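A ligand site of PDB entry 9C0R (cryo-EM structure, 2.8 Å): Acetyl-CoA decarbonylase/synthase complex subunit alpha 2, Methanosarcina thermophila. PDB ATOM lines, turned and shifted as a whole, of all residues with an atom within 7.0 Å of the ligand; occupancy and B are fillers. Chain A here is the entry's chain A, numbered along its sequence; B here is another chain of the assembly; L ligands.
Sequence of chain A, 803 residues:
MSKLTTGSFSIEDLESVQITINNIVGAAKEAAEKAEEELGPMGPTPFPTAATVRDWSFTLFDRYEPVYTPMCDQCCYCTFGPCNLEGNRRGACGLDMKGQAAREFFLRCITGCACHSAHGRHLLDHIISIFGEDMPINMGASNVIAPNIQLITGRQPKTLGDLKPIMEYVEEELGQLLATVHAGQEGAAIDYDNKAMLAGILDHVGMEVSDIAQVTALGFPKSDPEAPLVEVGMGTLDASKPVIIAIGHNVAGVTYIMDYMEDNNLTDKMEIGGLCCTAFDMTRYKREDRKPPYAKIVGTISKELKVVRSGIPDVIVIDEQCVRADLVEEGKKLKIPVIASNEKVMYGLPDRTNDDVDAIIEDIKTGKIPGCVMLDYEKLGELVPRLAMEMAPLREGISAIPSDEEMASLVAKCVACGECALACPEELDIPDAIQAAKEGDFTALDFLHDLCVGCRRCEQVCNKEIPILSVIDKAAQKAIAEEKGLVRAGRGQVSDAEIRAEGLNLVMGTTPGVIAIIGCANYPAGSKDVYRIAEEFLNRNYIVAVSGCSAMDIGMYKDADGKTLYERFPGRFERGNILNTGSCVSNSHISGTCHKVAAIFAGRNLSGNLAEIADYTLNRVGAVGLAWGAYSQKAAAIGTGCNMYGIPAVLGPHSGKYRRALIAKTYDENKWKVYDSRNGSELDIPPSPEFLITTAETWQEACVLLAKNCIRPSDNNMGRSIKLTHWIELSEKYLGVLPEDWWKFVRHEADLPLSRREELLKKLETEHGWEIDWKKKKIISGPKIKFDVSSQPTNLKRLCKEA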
ATOM      1  N   GLN A  74     -17.419  16.083  27.065  1.00  0.00           N
ATOM      2  CA  GLN A  74     -18.201  14.867  26.943  1.00  0.00           C
ATOM      3  C   GLN A  74     -19.629  15.195  26.530  1.00  0.00           C
ATOM      4  O   GLN A  74     -20.114  16.303  26.780  1.00  0.00           O
ATOM      5  CB  GLN A  74     -18.213  14.078  28.261  1.00  0.00           C
ATOM      6  CG  GLN A  74     -16.902  14.082  29.013  1.00  0.00           C
ATOM      7  CD  GLN A  74     -17.038  13.612  30.444  1.00  0.00           C
ATOM      8  OE1 GLN A  74     -16.038  13.401  31.136  1.00  0.00           O
ATOM      9  NE2 GLN A  74     -18.274  13.443  30.900  1.00  0.00           N
ATOM     10  N   CYS A  75     -20.283  14.228  25.911  1.00  0.00           N
ATOM     11  CA  CYS A  75     -21.713  14.280  25.657  1.00  0.00           C
ATOM     12  C   CYS A  75     -22.402  13.229  26.502  1.00  0.00           C
ATOM     13  O   CYS A  75     -21.876  12.132  26.706  1.00  0.00           O
ATOM     14  CB  CYS A  75     -22.053  14.074  24.179  1.00  0.00           C
ATOM     15  SG  CYS A  75     -23.808  13.813  23.848  1.00  0.00           S
ATOM     16  N   CYS A  76     -23.588  13.569  26.987  1.00  0.00           N
ATOM     17  CA  CYS A  76     -24.290  12.783  28.000  1.00  0.00           C
ATOM     18  C   CYS A  76     -25.770  12.636  27.668  1.00  0.00           C
ATOM     19  O   CYS A  76     -26.590  12.451  28.561  1.00  0.00           O
ATOM     20  CB  CYS A  76     -24.034  13.419  29.375  1.00  0.00           C
ATOM     21  SG  CYS A  76     -25.114  14.785  29.910  1.00  0.00           S
ATOM     22  N   TYR A  77     -26.106  12.670  26.379  1.00  0.00           N
ATOM     23  CA  TYR A  77     -27.504  12.708  25.962  1.00  0.00           C
ATOM     24  C   TYR A  77     -28.176  11.350  26.108  1.00  0.00           C
ATOM     25  O   TYR A  77     -29.333  11.270  26.556  1.00  0.00           O
ATOM     26  CB  TYR A  77     -27.607  13.191  24.514  1.00  0.00           C
ATOM     27  CG  TYR A  77     -27.705  14.696  24.381  1.00  0.00           C
ATOM     28  CD1 TYR A  77     -27.002  15.535  25.237  1.00  0.00           C
ATOM     29  CD2 TYR A  77     -28.507  15.270  23.402  1.00  0.00           C
ATOM     30  CE1 TYR A  77     -27.087  16.904  25.111  1.00  0.00           C
ATOM     31  CE2 TYR A  77     -28.605  16.641  23.281  1.00  0.00           C
ATOM     32  CZ  TYR A  77     -27.890  17.447  24.144  1.00  0.00           C
ATOM     33  OH  TYR A  77     -27.984  18.818  24.014  1.00  0.00           O
ATOM     34  N   CYS A  78     -27.497  10.269  25.730  1.00  0.00           N
ATOM     35  CA  CYS A  78     -28.102   8.943  25.707  1.00  0.00           C
ATOM     36  C   CYS A  78     -27.230   7.982  26.513  1.00  0.00           C
ATOM     37  O   CYS A  78     -26.148   8.334  26.982  1.00  0.00           O
ATOM     38  CB  CYS A  78     -28.298   8.444  24.271  1.00  0.00           C
ATOM     39  SG  CYS A  78     -26.832   7.761  23.482  1.00  0.00           S
ATOM     40  N   THR A  79     -27.733   6.756  26.673  1.00  0.00           N
ATOM     41  CA  THR A  79     -27.066   5.787  27.545  1.00  0.00           C
ATOM     42  C   THR A  79     -25.888   5.086  26.872  1.00  0.00           C
ATOM     43  O   THR A  79     -25.174   4.348  27.542  1.00  0.00           O
ATOM     44  CB  THR A  79     -28.044   4.742  28.060  1.00  0.00           C
ATOM     45  OG1 THR A  79     -28.212   3.704  27.090  1.00  0.00           O
ATOM     46  CG2 THR A  79     -29.395   5.370  28.360  1.00  0.00           C
ATOM     47  N   PHE A  80     -25.680   5.289  25.569  1.00  0.00           N
ATOM     48  CA  PHE A  80     -24.424   4.864  24.975  1.00  0.00           C
ATOM     49  C   PHE A  80     -23.251   5.606  25.594  1.00  0.00           C
ATOM     50  O   PHE A  80     -22.153   5.053  25.726  1.00  0.00           O
ATOM     51  CB  PHE A  80     -24.437   5.092  23.463  1.00  0.00           C
ATOM     52  CG  PHE A  80     -24.960   3.930  22.676  1.00  0.00           C
ATOM     53  CD1 PHE A  80     -24.343   2.694  22.749  1.00  0.00           C
ATOM     54  CD2 PHE A  80     -26.074   4.069  21.863  1.00  0.00           C
ATOM     55  CE1 PHE A  80     -24.835   1.623  22.032  1.00  0.00           C
ATOM     56  CE2 PHE A  80     -26.560   3.008  21.138  1.00  0.00           C
ATOM     57  CZ  PHE A  80     -25.937   1.780  21.224  1.00  0.00           C
ATOM     58  N   GLY A  81     -23.468   6.856  26.007  1.00  0.00           N
ATOM     59  CA  GLY A  81     -22.439   7.655  26.622  1.00  0.00           C
ATOM     60  C   GLY A  81     -22.306   7.388  28.104  1.00  0.00           C
ATOM     61  O   GLY A  81     -22.858   6.418  28.637  1.00  0.00           O
ATOM     62  N   PRO A  82     -21.570   8.252  28.809  1.00  0.00           N
ATOM     63  CA  PRO A  82     -20.950   9.501  28.328  1.00  0.00           C
ATOM     64  C   PRO A  82     -19.782   9.250  27.389  1.00  0.00           C
ATOM     65  O   PRO A  82     -18.958   8.372  27.613  1.00  0.00           O
ATOM     66  CB  PRO A  82     -20.514  10.181  29.635  1.00  0.00           C
ATOM     67  CG  PRO A  82     -20.200   9.037  30.548  1.00  0.00           C
ATOM     68  CD  PRO A  82     -21.229   7.984  30.215  1.00  0.00           C
ATOM     69  N   CYS A  83     -19.705  10.020  26.303  1.00  0.00           N
ATOM     70  CA  CYS A  83     -18.693   9.845  25.275  1.00  0.00           C
ATOM     71  C   CYS A  83     -17.662  10.956  25.375  1.00  0.00           C
ATOM     72  O   CYS A  83     -18.021  12.134  25.329  1.00  0.00           O
ATOM     73  CB  CYS A  83     -19.325   9.829  23.875  1.00  0.00           C
ATOM     74  SG  CYS A  83     -20.533   8.528  23.591  1.00  0.00           S
ATOM     75  N   ASN A  84     -16.395  10.587  25.498  1.00  0.00           N
ATOM     76  CA  ASN A  84     -15.321  11.563  25.543  1.00  0.00           C
ATOM     77  C   ASN A  84     -15.060  12.070  24.128  1.00  0.00           C
ATOM     78  O   ASN A  84     -14.698  11.298  23.236  1.00  0.00           O
ATOM     79  CB  ASN A  84     -14.061  10.935  26.145  1.00  0.00           C
ATOM     80  CG  ASN A  84     -12.981  11.953  26.426  1.00  0.00           C
ATOM     81  OD1 ASN A  84     -13.161  13.154  26.190  1.00  0.00           O
ATOM     82  ND2 ASN A  84     -11.859  11.499  26.947  1.00  0.00           N
ATOM     83  N   LEU A  85     -15.245  13.372  23.921  1.00  0.00           N
ATOM     84  CA  LEU A  85     -15.091  13.983  22.608  1.00  0.00           C
ATOM     85  C   LEU A  85     -13.896  14.935  22.535  1.00  0.00           C
ATOM     86  O   LEU A  85     -13.841  15.777  21.638  1.00  0.00           O
ATOM     87  CB  LEU A  85     -16.372  14.731  22.217  1.00  0.00           C
ATOM     88  CG  LEU A  85     -17.705  14.016  22.443  1.00  0.00           C
ATOM     89  CD1 LEU A  85     -18.851  15.009  22.394  1.00  0.00           C
ATOM     90  CD2 LEU A  85     -17.898  12.914  21.428  1.00  0.00           C
ATOM     91  N   ARG A  90     -15.294  11.651  17.908  1.00  0.00           N
ATOM     92  CA  ARG A  90     -16.696  11.350  17.672  1.00  0.00           C
ATOM     93  C   ARG A  90     -17.234  10.408  18.745  1.00  0.00           C
ATOM     94  O   ARG A  90     -16.505   9.584  19.301  1.00  0.00           O
ATOM     95  CB  ARG A  90     -16.898  10.736  16.289  1.00  0.00           C
ATOM     96  CG  ARG A  90     -16.707  11.724  15.157  1.00  0.00           C
ATOM     97  CD  ARG A  90     -16.826  11.063  13.793  1.00  0.00           C
ATOM     98  NE  ARG A  90     -16.550  11.990  12.715  1.00  0.00           N
ATOM     99  CZ  ARG A  90     -17.454  12.775  12.151  1.00  0.00           C
ATOM    100  NH1 ARG A  90     -18.712  12.768  12.538  1.00  0.00           N
ATOM    101  NH2 ARG A  90     -17.076  13.596  11.168  1.00  0.00           N
ATOM    102  N   GLY A  91     -18.528  10.567  19.046  1.00  0.00           N
ATOM    103  CA  GLY A  91     -19.193   9.718  20.001  1.00  0.00           C
ATOM    104  C   GLY A  91     -19.597   8.389  19.408  1.00  0.00           C
ATOM    105  O   GLY A  91     -19.283   8.050  18.275  1.00  0.00           O
ATOM    106  N   ALA A  92     -20.332   7.614  20.216  1.00  0.00           N
ATOM    107  CA  ALA A  92     -20.775   6.312  19.760  1.00  0.00           C
ATOM    108  C   ALA A  92     -21.782   6.415  18.621  1.00  0.00           C
ATOM    109  O   ALA A  92     -21.919   5.458  17.854  1.00  0.00           O
ATOM    110  CB  ALA A  92     -21.381   5.519  20.921  1.00  0.00           C
ATOM    111  N   CYS A  93     -22.475   7.537  18.491  1.00  0.00           N
ATOM    112  CA  CYS A  93     -23.406   7.756  17.387  1.00  0.00           C
ATOM    113  C   CYS A  93     -22.739   8.360  16.158  1.00  0.00           C
ATOM    114  O   CYS A  93     -23.395   8.484  15.123  1.00  0.00           O
ATOM    115  CB  CYS A  93     -24.557   8.652  17.837  1.00  0.00           C
ATOM    116  SG  CYS A  93     -24.067  10.283  18.412  1.00  0.00           S
ATOM    117  N   GLY A  94     -21.469   8.746  16.262  1.00  0.00           N
ATOM    118  CA  GLY A  94     -20.760   9.373  15.165  1.00  0.00           C
ATOM    119  C   GLY A  94     -20.700  10.878  15.197  1.00  0.00           C
ATOM    120  O   GLY A  94     -20.039  11.475  14.344  1.00  0.00           O
ATOM    121  N   LEU A  95     -21.372  11.518  16.152  1.00  0.00           N
ATOM    122  CA  LEU A  95     -21.343  12.971  16.270  1.00  0.00           C
ATOM    123  C   LEU A  95     -20.058  13.423  16.948  1.00  0.00           C
ATOM    124  O   LEU A  95     -19.585  12.788  17.900  1.00  0.00           O
ATOM    125  CB  LEU A  95     -22.556  13.465  17.062  1.00  0.00           C
ATOM    126  CG  LEU A  95     -22.805  14.977  17.055  1.00  0.00           C
ATOM    127  CD1 LEU A  95     -23.402  15.408  15.733  1.00  0.00           C
ATOM    128  CD2 LEU A  95     -23.704  15.369  18.202  1.00  0.00           C
ATOM    129  N   ASP A  96     -19.501  14.521  16.460  1.00  0.00           N
ATOM    130  CA  ASP A  96     -18.209  15.029  16.919  1.00  0.00           C
ATOM    131  C   ASP A  96     -18.407  16.183  17.898  1.00  0.00           C
ATOM    132  O   ASP A  96     -19.527  16.518  18.292  1.00  0.00           O
ATOM    133  CB  ASP A  96     -17.363  15.436  15.724  1.00  0.00           C
ATOM    134  CG  ASP A  96     -18.171  16.140  14.652  1.00  0.00           C
ATOM    135  OD1 ASP A  96     -19.321  15.723  14.407  1.00  0.00           O
ATOM    136  OD2 ASP A  96     -17.654  17.101  14.046  1.00  0.00           O
ATOM    137  N   GLN A 100     -21.761  18.463  18.611  1.00  0.00           N
ATOM    138  CA  GLN A 100     -22.369  18.462  19.940  1.00  0.00           C
ATOM    139  C   GLN A 100     -22.503  19.882  20.490  1.00  0.00           C
ATOM    140  O   GLN A 100     -23.525  20.213  21.100  1.00  0.00           O
ATOM    141  CB  GLN A 100     -21.549  17.582  20.886  1.00  0.00           C
ATOM    142  CG  GLN A 100     -21.950  17.707  22.358  1.00  0.00           C
ATOM    143  CD  GLN A 100     -23.350  17.193  22.648  1.00  0.00           C
ATOM    144  OE1 GLN A 100     -23.984  16.564  21.813  1.00  0.00           O
ATOM    145  NE2 GLN A 100     -23.840  17.486  23.842  1.00  0.00           N
ATOM    146  N   ARG A 103     -25.367  21.442  18.759  1.00  0.00           N
ATOM    147  CA  ARG A 103     -26.625  20.917  19.264  1.00  0.00           C
ATOM    148  C   ARG A 103     -26.981  21.511  20.618  1.00  0.00           C
ATOM    149  O   ARG A 103     -28.160  21.783  20.896  1.00  0.00           O
ATOM    150  CB  ARG A 103     -26.560  19.392  19.337  1.00  0.00           C
ATOM    151  CG  ARG A 103     -27.877  18.725  19.692  1.00  0.00           C
ATOM    152  CD  ARG A 103     -27.812  17.219  19.521  1.00  0.00           C
ATOM    153  NE  ARG A 103     -26.726  16.619  20.304  1.00  0.00           N
ATOM    154  CZ  ARG A 103     -26.502  15.320  20.386  1.00  0.00           C
ATOM    155  NH1 ARG A 103     -27.250  14.442  19.742  1.00  0.00           N
ATOM    156  NH2 ARG A 103     -25.478  14.888  21.114  1.00  0.00           N
ATOM    157  N   HIS A 182     -33.128  14.831  19.379  1.00  0.00           N
ATOM    158  CA  HIS A 182     -32.911  13.425  19.681  1.00  0.00           C
ATOM    159  C   HIS A 182     -31.561  12.934  19.190  1.00  0.00           C
ATOM    160  O   HIS A 182     -30.963  13.507  18.272  1.00  0.00           O
ATOM    161  CB  HIS A 182     -34.018  12.593  19.028  1.00  0.00           C
ATOM    162  CG  HIS A 182     -34.134  11.189  19.546  1.00  0.00           C
ATOM    163  ND1 HIS A 182     -33.491  10.129  18.972  1.00  0.00           N
ATOM    164  CD2 HIS A 182     -34.854  10.680  20.581  1.00  0.00           C
ATOM    165  CE1 HIS A 182     -33.792   9.023  19.630  1.00  0.00           C
ATOM    166  NE2 HIS A 182     -34.617   9.332  20.614  1.00  0.00           N
ATOM    167  N   ALA A 183     -31.079  11.864  19.817  1.00  0.00           N
ATOM    168  CA  ALA A 183     -29.827  11.252  19.402  1.00  0.00           C
ATOM    169  C   ALA A 183     -29.956  10.668  18.000  1.00  0.00           C
ATOM    170  O   ALA A 183     -30.959  10.038  17.662  1.00  0.00           O
ATOM    171  CB  ALA A 183     -29.412  10.157  20.387  1.00  0.00           C
ATOM    172  N   GLY A 184     -28.937  10.893  17.181  1.00  0.00           N
ATOM    173  CA  GLY A 184     -28.961  10.440  15.806  1.00  0.00           C
ATOM    174  C   GLY A 184     -29.989  11.117  14.939  1.00  0.00           C
ATOM    175  O   GLY A 184     -30.631  10.459  14.110  1.00  0.00           O
ATOM    176  N   ARG B 457     -15.813   3.573  18.737  1.00  0.00           N
ATOM    177  CA  ARG B 457     -15.195   4.437  19.729  1.00  0.00           C
ATOM    178  C   ARG B 457     -13.816   3.935  20.143  1.00  0.00           C
ATOM    179  O   ARG B 457     -13.026   4.699  20.697  1.00  0.00           O
ATOM    180  CB  ARG B 457     -16.088   4.576  20.961  1.00  0.00           C
ATOM    181  CG  ARG B 457     -16.716   5.961  21.115  1.00  0.00           C
ATOM    182  CD  ARG B 457     -17.842   5.984  22.145  1.00  0.00           C
ATOM    183  NE  ARG B 457     -17.463   5.353  23.407  1.00  0.00           N
ATOM    184  CZ  ARG B 457     -18.193   5.400  24.519  1.00  0.00           C
ATOM    185  NH1 ARG B 457     -19.343   6.052  24.560  1.00  0.00           N
ATOM    186  NH2 ARG B 457     -17.762   4.773  25.606  1.00  0.00           N
ATOM    187  N   TYR B 631     -31.546   3.012  25.001  1.00  0.00           N
ATOM    188  CA  TYR B 631     -30.547   4.070  25.075  1.00  0.00           C
ATOM    189  C   TYR B 631     -31.153   5.435  24.761  1.00  0.00           C
ATOM    190  O   TYR B 631     -30.692   6.454  25.286  1.00  0.00           O
ATOM    191  CB  TYR B 631     -29.367   3.786  24.142  1.00  0.00           C
ATOM    192  CG  TYR B 631     -29.693   3.934  22.678  1.00  0.00           C
ATOM    193  CD1 TYR B 631     -29.649   5.175  22.049  1.00  0.00           C
ATOM    194  CD2 TYR B 631     -30.053   2.843  21.914  1.00  0.00           C
ATOM    195  CE1 TYR B 631     -29.963   5.311  20.714  1.00  0.00           C
ATOM    196  CE2 TYR B 631     -30.364   2.967  20.592  1.00  0.00           C
ATOM    197  CZ  TYR B 631     -30.324   4.207  19.995  1.00  0.00           C
ATOM    198  OH  TYR B 631     -30.632   4.321  18.663  1.00  0.00           O
ATOM    199  N   GLN B 633     -33.965   8.644  23.880  1.00  0.00           N
ATOM    200  CA  GLN B 633     -34.942   9.424  24.639  1.00  0.00           C
ATOM    201  C   GLN B 633     -36.358   8.942  24.398  1.00  0.00           C
ATOM    202  O   GLN B 633     -37.219   9.061  25.278  1.00  0.00           O
ATOM    203  CB  GLN B 633     -34.810  10.904  24.284  1.00  0.00           C
ATOM    204  CG  GLN B 633     -33.457  11.511  24.637  1.00  0.00           C
ATOM    205  CD  GLN B 633     -32.530  11.608  23.442  1.00  0.00           C
ATOM    206  OE1 GLN B 633     -32.540  10.759  22.557  1.00  0.00           O
ATOM    207  NE2 GLN B 633     -31.717  12.657  23.403  1.00  0.00           N
HETATM  208 FE1  LIG L   1     -22.479   9.452  22.851  1.00  0.00          FE
HETATM  209 FE2  LIG L   1     -23.960  10.236  20.691  1.00  0.00          FE
HETATM  210 FE3  LIG L   1     -24.000  11.711  22.991  1.00  0.00          FE
HETATM  211 FE4  LIG L   1     -25.211   9.255  22.920  1.00  0.00          FE
HETATM  212  S1  LIG L   1     -25.798  11.110  21.719  1.00  0.00           S
HETATM  213  S2  LIG L   1     -23.854  10.080  24.563  1.00  0.00           S
HETATM  214  S3  LIG L   1     -23.788   8.125  21.537  1.00  0.00           S
HETATM  215  S4  LIG L   1     -22.204  11.349  21.625  1.00  0.00           S
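N of Gly 81 lies close to S2 of the ligand, at 3.6 Å. SG of Cys 78 is bound to FE4 of the ligand. S3 of the ligand sits close to N of Ala 92, at 3.7 Å. The side-chain sulfur (SG) of Cys 83 is bound to an iron atom (FE1) of the ligand, 2.3 Å away. An iron atom (FE2) of the ligand is bound by the side-chain sulfur (SG) of Cys 93 (2.3 Å). The backbone NH of Cys 93 sits close to a sulfur (S3) of the ligand (3.4 Å). An iron atom (FE3) of the ligand is bound by the side-chain sulfur (SG) of Cys 75, 2.3 Å away.
Merely in contact with the ligand: Tyr 77, Phe 80, Gly 91, Arg 103 and Ala 183. Hydrophobic or aromatic side chains within 4 Å of the ligand: Tyr 77, Phe 80, Ala 92 and Ala 183. Of the 27 residues printed, 11 come within 4 Å of the ligand. The nearest printed residue that does not touch the ligand is Cys 76 (4.3 Å).
NE of Arg 103 sits at hydrogen-bond distance from OE1 of Gln 100 (3.1 Å). O of Cys 75 lies within hydrogen-bond range of N of Cys 83, at 3.1 Å. The side-chain sulfur (SG) of Cys 83 sits close to the backbone NH (N) of Ala 92, 3.5 Å away. NH2 of Arg 103 sits close to SG of Cys 75 (3.4 Å). SG of Cys 78 lies close to N of Phe 80. NH1 of Arg 457 of chain B is in hydrogen-bond range of O of Phe 80. The side-chain sulfur (SG) of Cys 93 sits close to the backbone NH (N) of Leu 95, at 3.7 Å. NH1 of Arg 457 of chain B lies close to SG of Cys 83 (2.9 Å).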
